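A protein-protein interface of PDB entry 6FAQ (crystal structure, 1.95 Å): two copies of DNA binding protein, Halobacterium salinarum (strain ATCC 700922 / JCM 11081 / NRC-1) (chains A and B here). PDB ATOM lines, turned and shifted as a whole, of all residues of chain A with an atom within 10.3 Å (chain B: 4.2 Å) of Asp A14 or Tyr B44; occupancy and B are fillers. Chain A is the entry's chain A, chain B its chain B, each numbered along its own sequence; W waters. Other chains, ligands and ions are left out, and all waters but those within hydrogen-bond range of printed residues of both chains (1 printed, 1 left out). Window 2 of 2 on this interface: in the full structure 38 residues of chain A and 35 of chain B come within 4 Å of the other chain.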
ATOM      1  N   ASP A  11      21.105 -33.874 -34.905  1.00  0.00           N
ATOM      2  CA  ASP A  11      21.640 -33.956 -33.551  1.00  0.00           C
ATOM      3  C   ASP A  11      20.770 -33.147 -32.594  1.00  0.00           C
ATOM      4  O   ASP A  11      20.160 -32.152 -32.987  1.00  0.00           O
ATOM      5  CB  ASP A  11      23.084 -33.453 -33.513  1.00  0.00           C
ATOM      6  CG  ASP A  11      23.813 -33.868 -32.250  1.00  0.00           C
ATOM      7  OD1 ASP A  11      24.069 -35.080 -32.079  1.00  0.00           O
ATOM      8  OD2 ASP A  11      24.135 -32.985 -31.428  1.00  0.00           O
ATOM      9  N   ALA A  12      20.715 -33.581 -31.334  1.00  0.00           N
ATOM     10  CA  ALA A  12      19.911 -32.880 -30.341  1.00  0.00           C
ATOM     11  C   ALA A  12      20.527 -31.549 -29.936  1.00  0.00           C
ATOM     12  O   ALA A  12      19.822 -30.696 -29.383  1.00  0.00           O
ATOM     13  CB  ALA A  12      19.719 -33.760 -29.105  1.00  0.00           C
ATOM     14  N   ARG A  13      21.819 -31.345 -30.198  1.00  0.00           N
ATOM     15  CA  ARG A  13      22.463 -30.088 -29.841  1.00  0.00           C
ATOM     16  C   ARG A  13      22.041 -28.934 -30.743  1.00  0.00           C
ATOM     17  O   ARG A  13      22.380 -27.785 -30.443  1.00  0.00           O
ATOM     18  CB  ARG A  13      23.985 -30.257 -29.874  1.00  0.00           C
ATOM     19  CG  ARG A  13      24.510 -31.213 -28.808  1.00  0.00           C
ATOM     20  CD  ARG A  13      26.033 -31.252 -28.763  1.00  0.00           C
ATOM     21  NE  ARG A  13      26.522 -31.977 -27.591  1.00  0.00           N
ATOM     22  CZ  ARG A  13      27.806 -32.121 -27.274  1.00  0.00           C
ATOM     23  NH1 ARG A  13      28.751 -31.592 -28.039  1.00  0.00           N
ATOM     24  NH2 ARG A  13      28.146 -32.798 -26.186  1.00  0.00           N
ATOM     25  N   ASP A  14      21.305 -29.205 -31.820  1.00  0.00           N
ATOM     26  CA  ASP A  14      20.824 -28.167 -32.722  1.00  0.00           C
ATOM     27  C   ASP A  14      19.396 -27.727 -32.420  1.00  0.00           C
ATOM     28  O   ASP A  14      18.861 -26.872 -33.133  1.00  0.00           O
ATOM     29  CB  ASP A  14      20.913 -28.654 -34.173  1.00  0.00           C
ATOM     30  CG  ASP A  14      22.329 -29.013 -34.578  1.00  0.00           C
ATOM     31  OD1 ASP A  14      23.273 -28.402 -34.035  1.00  0.00           O
ATOM     32  OD2 ASP A  14      22.498 -29.904 -35.438  1.00  0.00           O
ATOM     33  N   LEU A  15      18.770 -28.281 -31.384  1.00  0.00           N
ATOM     34  CA  LEU A  15      17.409 -27.900 -31.034  1.00  0.00           C
ATOM     35  C   LEU A  15      17.340 -26.423 -30.654  1.00  0.00           C
ATOM     36  O   LEU A  15      18.327 -25.812 -30.233  1.00  0.00           O
ATOM     37  CB  LEU A  15      16.900 -28.753 -29.873  1.00  0.00           C
ATOM     38  CG  LEU A  15      16.815 -30.260 -30.121  1.00  0.00           C
ATOM     39  CD1 LEU A  15      16.530 -30.989 -28.819  1.00  0.00           C
ATOM     40  CD2 LEU A  15      15.751 -30.579 -31.162  1.00  0.00           C
ATOM     41  N   THR A  16      16.150 -25.847 -30.805  1.00  0.00           N
ATOM     42  CA  THR A  16      15.922 -24.478 -30.366  1.00  0.00           C
ATOM     43  C   THR A  16      15.866 -24.416 -28.843  1.00  0.00           C
ATOM     44  O   THR A  16      15.672 -25.424 -28.159  1.00  0.00           O
ATOM     45  CB  THR A  16      14.618 -23.924 -30.943  1.00  0.00           C
ATOM     46  OG1 THR A  16      13.509 -24.657 -30.408  1.00  0.00           O
ATOM     47  CG2 THR A  16      14.610 -24.023 -32.460  1.00  0.00           C
ATOM     48  N   ALA A  17      16.036 -23.205 -28.310  1.00  0.00           N
ATOM     49  CA  ALA A  17      15.948 -23.021 -26.866  1.00  0.00           C
ATOM     50  C   ALA A  17      14.581 -23.446 -26.348  1.00  0.00           C
ATOM     51  O   ALA A  17      14.474 -24.071 -25.287  1.00  0.00           O
ATOM     52  CB  ALA A  17      16.228 -21.563 -26.501  1.00  0.00           C
ATOM     53  N   PHE A  18      13.524 -23.125 -27.098  1.00  0.00           N
ATOM     54  CA  PHE A  18      12.174 -23.508 -26.697  1.00  0.00           C
ATOM     55  C   PHE A  18      12.023 -25.024 -26.661  1.00  0.00           C
ATOM     56  O   PHE A  18      11.414 -25.574 -25.736  1.00  0.00           O
ATOM     57  CB  PHE A  18      11.163 -22.880 -27.660  1.00  0.00           C
ATOM     58  CG  PHE A  18       9.727 -23.127 -27.294  1.00  0.00           C
ATOM     59  CD1 PHE A  18       9.105 -22.364 -26.318  1.00  0.00           C
ATOM     60  CD2 PHE A  18       8.993 -24.103 -27.942  1.00  0.00           C
ATOM     61  CE1 PHE A  18       7.781 -22.585 -25.988  1.00  0.00           C
ATOM     62  CE2 PHE A  18       7.671 -24.327 -27.616  1.00  0.00           C
ATOM     63  CZ  PHE A  18       7.064 -23.567 -26.637  1.00  0.00           C
ATOM     64  N   GLN A  19      12.579 -25.717 -27.657  1.00  0.00           N
ATOM     65  CA  GLN A  19      12.496 -27.173 -27.683  1.00  0.00           C
ATOM     66  C   GLN A  19      13.313 -27.795 -26.556  1.00  0.00           C
ATOM     67  O   GLN A  19      12.858 -28.744 -25.907  1.00  0.00           O
ATOM     68  CB  GLN A  19      12.964 -27.695 -29.042  1.00  0.00           C
ATOM     69  CG  GLN A  19      12.007 -27.375 -30.180  1.00  0.00           C
ATOM     70  CD  GLN A  19      12.573 -27.733 -31.539  1.00  0.00           C
ATOM     71  OE1 GLN A  19      13.785 -27.901 -31.697  1.00  0.00           O
ATOM     72  NE2 GLN A  19      11.697 -27.854 -32.530  1.00  0.00           N
ATOM     73  N   LYS A  20      14.522 -27.279 -26.312  1.00  0.00           N
ATOM     74  CA  LYS A  20      15.325 -27.780 -25.202  1.00  0.00           C
ATOM     75  C   LYS A  20      14.629 -27.566 -23.866  1.00  0.00           C
ATOM     76  O   LYS A  20      14.773 -28.386 -22.952  1.00  0.00           O
ATOM     77  CB  LYS A  20      16.696 -27.100 -25.192  1.00  0.00           C
ATOM     78  CG  LYS A  20      17.587 -27.476 -26.367  1.00  0.00           C
ATOM     79  CD  LYS A  20      18.939 -26.769 -26.292  1.00  0.00           C
ATOM     80  CE  LYS A  20      19.840 -27.151 -27.457  1.00  0.00           C
ATOM     81  NZ  LYS A  20      21.151 -26.433 -27.415  1.00  0.00           N
ATOM     82  N   LEU A  23      12.137 -30.333 -23.288  1.00  0.00           N
ATOM     83  CA  LEU A  23      12.816 -31.532 -22.808  1.00  0.00           C
ATOM     84  C   LEU A  23      13.183 -31.395 -21.337  1.00  0.00           C
ATOM     85  O   LEU A  23      13.056 -32.352 -20.565  1.00  0.00           O
ATOM     86  CB  LEU A  23      14.063 -31.809 -23.648  1.00  0.00           C
ATOM     87  CG  LEU A  23      13.847 -32.022 -25.147  1.00  0.00           C
ATOM     88  CD1 LEU A  23      15.162 -32.395 -25.821  1.00  0.00           C
ATOM     89  CD2 LEU A  23      12.789 -33.083 -25.412  1.00  0.00           C
ATOM     90  N   ASN A  56       5.779 -27.727 -31.837  1.00  0.00           N
ATOM     91  CA  ASN A  56       7.116 -28.111 -31.402  1.00  0.00           C
ATOM     92  C   ASN A  56       7.105 -29.461 -30.694  1.00  0.00           C
ATOM     93  O   ASN A  56       8.042 -30.251 -30.853  1.00  0.00           O
ATOM     94  CB  ASN A  56       7.702 -27.033 -30.492  1.00  0.00           C
ATOM     95  CG  ASN A  56       8.378 -25.923 -31.272  1.00  0.00           C
ATOM     96  OD1 ASN A  56       9.525 -26.063 -31.697  1.00  0.00           O
ATOM     97  ND2 ASN A  56       7.672 -24.816 -31.466  1.00  0.00           N
ATOM     98  N   LEU A  60       9.396 -32.722 -31.652  1.00  0.00           N
ATOM     99  CA  LEU A  60      10.192 -33.528 -30.733  1.00  0.00           C
ATOM    100  C   LEU A  60       9.787 -34.996 -30.781  1.00  0.00           C
ATOM    101  O   LEU A  60      10.633 -35.880 -30.600  1.00  0.00           O
ATOM    102  CB  LEU A  60      10.057 -32.984 -29.311  1.00  0.00           C
ATOM    103  CG  LEU A  60      10.696 -31.617 -29.059  1.00  0.00           C
ATOM    104  CD1 LEU A  60      10.341 -31.104 -27.670  1.00  0.00           C
ATOM    105  CD2 LEU A  60      12.205 -31.689 -29.232  1.00  0.00           C
ATOM    106  N   LYS A  63      11.337 -36.509 -33.949  1.00  0.00           N
ATOM    107  CA  LYS A  63      12.769 -36.706 -33.762  1.00  0.00           C
ATOM    108  C   LYS A  63      13.087 -37.868 -32.830  1.00  0.00           C
ATOM    109  O   LYS A  63      14.266 -38.197 -32.663  1.00  0.00           O
ATOM    110  CB  LYS A  63      13.407 -35.428 -33.213  1.00  0.00           C
ATOM    111  CG  LYS A  63      13.329 -34.234 -34.154  1.00  0.00           C
ATOM    112  CD  LYS A  63      13.758 -32.949 -33.453  1.00  0.00           C
ATOM    113  CE  LYS A  63      13.685 -31.745 -34.384  1.00  0.00           C
ATOM    114  NZ  LYS A  63      14.644 -31.848 -35.519  1.00  0.00           N
ATOM    115  N   LEU A  65      12.594 -37.910 -29.567  1.00  0.00           N
ATOM    116  CA  LEU A  65      13.008 -37.427 -28.256  1.00  0.00           C
ATOM    117  C   LEU A  65      11.881 -37.451 -27.234  1.00  0.00           C
ATOM    118  O   LEU A  65      12.152 -37.539 -26.030  1.00  0.00           O
ATOM    119  CB  LEU A  65      13.553 -36.000 -28.373  1.00  0.00           C
ATOM    120  CG  LEU A  65      14.746 -35.826 -29.316  1.00  0.00           C
ATOM    121  CD1 LEU A  65      15.115 -34.359 -29.436  1.00  0.00           C
ATOM    122  CD2 LEU A  65      15.940 -36.641 -28.839  1.00  0.00           C
ATOM    123  N   ALA A  87      19.668 -36.504 -24.419  1.00  0.00           N
ATOM    124  CA  ALA A  87      19.853 -35.130 -24.870  1.00  0.00           C
ATOM    125  C   ALA A  87      19.868 -34.162 -23.694  1.00  0.00           C
ATOM    126  O   ALA A  87      20.632 -33.189 -23.691  1.00  0.00           O
ATOM    127  CB  ALA A  87      18.753 -34.754 -25.862  1.00  0.00           C
ATOM    128  N   ASP A  90      23.190 -34.736 -21.893  1.00  0.00           N
ATOM    129  CA  ASP A  90      24.309 -34.259 -22.700  1.00  0.00           C
ATOM    130  C   ASP A  90      24.502 -32.757 -22.537  1.00  0.00           C
ATOM    131  O   ASP A  90      25.619 -32.285 -22.296  1.00  0.00           O
ATOM    132  CB  ASP A  90      24.079 -34.618 -24.168  1.00  0.00           C
ATOM    133  CG  ASP A  90      25.136 -34.035 -25.082  1.00  0.00           C
ATOM    134  OD1 ASP A  90      26.301 -34.475 -25.000  1.00  0.00           O
ATOM    135  OD2 ASP A  90      24.800 -33.135 -25.882  1.00  0.00           O
ATOM    136  N   ASP A  91      23.420 -31.987 -22.664  1.00  0.00           N
ATOM    137  CA  ASP A  91      23.532 -30.540 -22.518  1.00  0.00           C
ATOM    138  C   ASP A  91      23.874 -30.146 -21.089  1.00  0.00           C
ATOM    139  O   ASP A  91      24.595 -29.164 -20.877  1.00  0.00           O
ATOM    140  CB  ASP A  91      22.236 -29.861 -22.960  1.00  0.00           C
ATOM    141  CG  ASP A  91      22.140 -29.719 -24.469  1.00  0.00           C
ATOM    142  OD1 ASP A  91      23.066 -30.177 -25.174  1.00  0.00           O
ATOM    143  OD2 ASP A  91      21.142 -29.142 -24.952  1.00  0.00           O
ATOM    144  N   TRP A  94      27.648 -30.670 -20.633  1.00  0.00           N
ATOM    145  CA  TRP A  94      28.414 -29.611 -21.280  1.00  0.00           C
ATOM    146  C   TRP A  94      28.301 -28.308 -20.499  1.00  0.00           C
ATOM    147  O   TRP A  94      29.308 -27.636 -20.246  1.00  0.00           O
ATOM    148  CB  TRP A  94      27.941 -29.422 -22.721  1.00  0.00           C
ATOM    149  CG  TRP A  94      28.781 -28.450 -23.493  1.00  0.00           C
ATOM    150  CD1 TRP A  94      30.030 -28.668 -23.998  1.00  0.00           C
ATOM    151  CD2 TRP A  94      28.433 -27.107 -23.849  1.00  0.00           C
ATOM    152  NE1 TRP A  94      30.481 -27.543 -24.645  1.00  0.00           N
ATOM    153  CE2 TRP A  94      29.519 -26.572 -24.570  1.00  0.00           C
ATOM    154  CE3 TRP A  94      27.307 -26.308 -23.630  1.00  0.00           C
ATOM    155  CZ2 TRP A  94      29.514 -25.272 -25.071  1.00  0.00           C
ATOM    156  CZ3 TRP A  94      27.304 -25.019 -24.128  1.00  0.00           C
ATOM    157  CH2 TRP A  94      28.401 -24.514 -24.841  1.00  0.00           C
ATOM    158  N   LYS A  98      31.544 -26.269 -18.488  1.00  0.00           N
ATOM    159  CA  LYS A  98      31.966 -24.885 -18.643  1.00  0.00           C
ATOM    160  C   LYS A  98      31.788 -24.071 -17.370  1.00  0.00           C
ATOM    161  O   LYS A  98      32.541 -23.114 -17.147  1.00  0.00           O
ATOM    162  CB  LYS A  98      31.188 -24.218 -19.783  1.00  0.00           C
ATOM    163  CG  LYS A  98      31.364 -24.890 -21.140  1.00  0.00           C
ATOM    164  CD  LYS A  98      32.806 -24.823 -21.625  1.00  0.00           C
ATOM    165  CE  LYS A  98      32.965 -25.469 -22.992  1.00  0.00           C
ATOM    166  NZ  LYS A  98      34.386 -25.474 -23.442  1.00  0.00           N
ATOM    167  N   PHE B  18      21.748 -20.514 -29.574  1.00  0.00           N
ATOM    168  CA  PHE B  18      23.098 -20.142 -29.982  1.00  0.00           C
ATOM    169  C   PHE B  18      23.657 -19.053 -29.075  1.00  0.00           C
ATOM    170  O   PHE B  18      24.807 -19.131 -28.627  1.00  0.00           O
ATOM    171  CB  PHE B  18      23.098 -19.687 -31.440  1.00  0.00           C
ATOM    172  CG  PHE B  18      24.469 -19.409 -31.985  1.00  0.00           C
ATOM    173  CD1 PHE B  18      25.296 -20.448 -32.381  1.00  0.00           C
ATOM    174  CD2 PHE B  18      24.931 -18.112 -32.099  1.00  0.00           C
ATOM    175  CE1 PHE B  18      26.559 -20.194 -32.883  1.00  0.00           C
ATOM    176  CE2 PHE B  18      26.191 -17.854 -32.603  1.00  0.00           C
ATOM    177  CZ  PHE B  18      27.007 -18.897 -32.991  1.00  0.00           C
ATOM    178  N   ASN B  21      24.518 -20.455 -25.742  1.00  0.00           N
ATOM    179  CA  ASN B  21      25.753 -21.231 -25.784  1.00  0.00           C
ATOM    180  C   ASN B  21      26.976 -20.325 -25.760  1.00  0.00           C
ATOM    181  O   ASN B  21      28.005 -20.691 -25.183  1.00  0.00           O
ATOM    182  CB  ASN B  21      25.765 -22.131 -27.018  1.00  0.00           C
ATOM    183  CG  ASN B  21      24.764 -23.270 -26.920  1.00  0.00           C
ATOM    184  OD1 ASN B  21      24.346 -23.653 -25.827  1.00  0.00           O
ATOM    185  ND2 ASN B  21      24.381 -23.820 -28.066  1.00  0.00           N
ATOM    186  N   LEU B  40      32.466 -23.445 -29.598  1.00  0.00           N
ATOM    187  CA  LEU B  40      31.150 -23.764 -30.141  1.00  0.00           C
ATOM    188  C   LEU B  40      31.231 -24.892 -31.160  1.00  0.00           C
ATOM    189  O   LEU B  40      30.374 -25.782 -31.176  1.00  0.00           O
ATOM    190  CB  LEU B  40      30.530 -22.515 -30.767  1.00  0.00           C
ATOM    191  CG  LEU B  40      30.220 -21.380 -29.790  1.00  0.00           C
ATOM    192  CD1 LEU B  40      29.844 -20.113 -30.538  1.00  0.00           C
ATOM    193  CD2 LEU B  40      29.108 -21.790 -28.836  1.00  0.00           C
ATOM    194  N   GLU B  41      32.256 -24.877 -32.016  1.00  0.00           N
ATOM    195  CA  GLU B  41      32.388 -25.927 -33.022  1.00  0.00           C
ATOM    196  C   GLU B  41      32.623 -27.284 -32.372  1.00  0.00           C
ATOM    197  O   GLU B  41      32.136 -28.309 -32.863  1.00  0.00           O
ATOM    198  CB  GLU B  41      33.521 -25.589 -33.992  1.00  0.00           C
ATOM    199  CG  GLU B  41      33.171 -24.468 -34.957  1.00  0.00           C
ATOM    200  CD  GLU B  41      34.282 -24.165 -35.948  1.00  0.00           C
ATOM    201  OE1 GLU B  41      35.443 -24.545 -35.687  1.00  0.00           O
ATOM    202  OE2 GLU B  41      33.985 -23.547 -36.991  1.00  0.00           O
ATOM    203  N   GLU B  42      33.373 -27.314 -31.269  1.00  0.00           N
ATOM    204  CA  GLU B  42      33.553 -28.566 -30.545  1.00  0.00           C
ATOM    205  C   GLU B  42      32.240 -29.052 -29.949  1.00  0.00           C
ATOM    206  O   GLU B  42      32.015 -30.264 -29.851  1.00  0.00           O
ATOM    207  CB  GLU B  42      34.604 -28.396 -29.449  1.00  0.00           C
ATOM    208  CG  GLU B  42      34.910 -29.677 -28.690  1.00  0.00           C
ATOM    209  CD  GLU B  42      36.176 -29.577 -27.861  1.00  0.00           C
ATOM    210  OE1 GLU B  42      36.820 -28.506 -27.883  1.00  0.00           O
ATOM    211  OE2 GLU B  42      36.528 -30.571 -27.191  1.00  0.00           O
ATOM    212  N   TYR B  43      31.359 -28.129 -29.556  1.00  0.00           N
ATOM    213  CA  TYR B  43      30.061 -28.522 -29.019  1.00  0.00           C
ATOM    214  C   TYR B  43      29.132 -29.005 -30.126  1.00  0.00           C
ATOM    215  O   TYR B  43      28.565 -30.101 -30.041  1.00  0.00           O
ATOM    216  CB  TYR B  43      29.431 -27.352 -28.262  1.00  0.00           C
ATOM    217  CG  TYR B  43      27.975 -27.570 -27.910  1.00  0.00           C
ATOM    218  CD1 TYR B  43      27.613 -28.352 -26.819  1.00  0.00           C
ATOM    219  CD2 TYR B  43      26.962 -26.996 -28.668  1.00  0.00           C
ATOM    220  CE1 TYR B  43      26.283 -28.555 -26.493  1.00  0.00           C
ATOM    221  CE2 TYR B  43      25.630 -27.193 -28.350  1.00  0.00           C
ATOM    222  CZ  TYR B  43      25.296 -27.974 -27.262  1.00  0.00           C
ATOM    223  OH  TYR B  43      23.971 -28.175 -26.941  1.00  0.00           O
ATOM    224  N   TYR B  44      28.958 -28.197 -31.175  1.00  0.00           N
ATOM    225  CA  TYR B  44      28.038 -28.558 -32.245  1.00  0.00           C
ATOM    226  C   TYR B  44      28.556 -29.701 -33.106  1.00  0.00           C
ATOM    227  O   TYR B  44      27.757 -30.362 -33.777  1.00  0.00           O
ATOM    228  CB  TYR B  44      27.755 -27.348 -33.138  1.00  0.00           C
ATOM    229  CG  TYR B  44      26.883 -26.284 -32.503  1.00  0.00           C
ATOM    230  CD1 TYR B  44      25.533 -26.512 -32.267  1.00  0.00           C
ATOM    231  CD2 TYR B  44      27.408 -25.047 -32.156  1.00  0.00           C
ATOM    232  CE1 TYR B  44      24.731 -25.538 -31.693  1.00  0.00           C
ATOM    233  CE2 TYR B  44      26.617 -24.070 -31.584  1.00  0.00           C
ATOM    234  CZ  TYR B  44      25.280 -24.319 -31.354  1.00  0.00           C
ATOM    235  OH  TYR B  44      24.500 -23.338 -30.785  1.00  0.00           O
ATOM    236  N   GLY B  45      29.864 -29.952 -33.107  1.00  0.00           N
ATOM    237  CA  GLY B  45      30.405 -30.933 -34.023  1.00  0.00           C
ATOM    238  C   GLY B  45      30.323 -30.524 -35.474  1.00  0.00           C
ATOM    239  O   GLY B  45      30.446 -31.376 -36.360  1.00  0.00           O
ATOM    240  N   GLU B  46      30.106 -29.237 -35.742  1.00  0.00           N
ATOM    241  CA  GLU B  46      30.020 -28.714 -37.096  1.00  0.00           C
ATOM    242  C   GLU B  46      30.632 -27.322 -37.121  1.00  0.00           C
ATOM    243  O   GLU B  46      30.747 -26.655 -36.089  1.00  0.00           O
ATOM    244  CB  GLU B  46      28.569 -28.652 -37.596  1.00  0.00           C
ATOM    245  CG  GLU B  46      27.827 -29.980 -37.554  1.00  0.00           C
ATOM    246  CD  GLU B  46      28.390 -31.000 -38.525  1.00  0.00           C
ATOM    247  OE1 GLU B  46      29.304 -30.646 -39.302  1.00  0.00           O
ATOM    248  OE2 GLU B  46      27.919 -32.157 -38.513  1.00  0.00           O
ATOM    249  N   VAL B  48      31.133 -23.462 -37.354  1.00  0.00           N
ATOM    250  CA  VAL B  48      30.359 -22.282 -36.984  1.00  0.00           C
ATOM    251  C   VAL B  48      30.837 -21.131 -37.858  1.00  0.00           C
ATOM    252  O   VAL B  48      32.021 -20.772 -37.832  1.00  0.00           O
ATOM    253  CB  VAL B  48      30.510 -21.946 -35.493  1.00  0.00           C
ATOM    254  CG1 VAL B  48      29.906 -20.582 -35.188  1.00  0.00           C
ATOM    255  CG2 VAL B  48      29.860 -23.026 -34.636  1.00  0.00           C
HETATM  256  O   HOH W   1      25.153 -30.341 -33.875  1.00  0.00           O
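Of the 10 printed residues of chain B, 4 touch a printed residue of chain A. Among the printed residues, 8 pairs touch across the chains. Among the printed residues, no Asp or Glu carboxylate lies within 4 Å of a Lys or Arg side-chain nitrogen of the other chain.
Water W1 lies within hydrogen-bond range of the backbone carbonyl oxygen (O) of Tyr B44 and the side-chain carboxylate (OD1) of Asp A14.
NH1 of Arg A13 lies within hydrogen-bond range of O of Tyr B43 (2.5 Å). The side-chain hydroxyl of Tyr B43 lies within hydrogen-bond range of the side-chain amino group of Lys A20 (3.3 Å). The side-chain carboxylate of Asp A91 lies within hydrogen-bond range of the side-chain hydroxyl of Tyr B43 (2.8 Å).
Of chain B, only Tyr B44 comes within 4 Å of Asp A14. Of the printed residues of chain B, Asp A91 touches Tyr B43. Of the printed residues of chain B, Trp A94 touches Asn B21 and Tyr B43. No residue of chain A comes within 4 Å of Leu B40. Tyr B43 touches just these residues of chain A: Arg A13, Lys A20, Asp A91 and Trp A94. Of chain A, only Arg A13 (3.5 Å) and Asp A14 (3.4 Å) come within 4 Å of Tyr B44. Gly B45 touches none of the printed residues of chain A. No residue of chain A comes within 4 Å of Glu B46. Val B48 touches none of the printed residues of chain A. The nearest printed residue of chain B that does not touch Asp A14 is Tyr B43 (5.7 Å).
Among the printed residues, pairs that only touch across the chains: Trp A94 with Tyr B43, Asp A14 with Tyr B44, Arg A13 with Tyr B44, Trp A94 with Asn B21 and Arg A13 with Glu B42.
1 position is printed for both chains. Of the 8 pairs that touch across the chains among the printed residues, none has its exchanged pair printed and touching as well.
The backbone NH of Arg A13 lies within hydrogen-bond range of the side-chain carboxylate of Asp A11. The side-chain carboxylate (OD2) of Asp A90 is in salt-bridge range of the guanidinium group (NE) of Arg A13, at 2.7 Å. The side-chain carboxylate of Asp A91 is in salt-bridge range of the side-chain amino group of Lys A20 (3.7 Å). The side-chain amide nitrogen (ND2) of Asn B21 sits at hydrogen-bond distance from the side-chain hydroxyl (OH) of Tyr B44 (2.8 Å).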
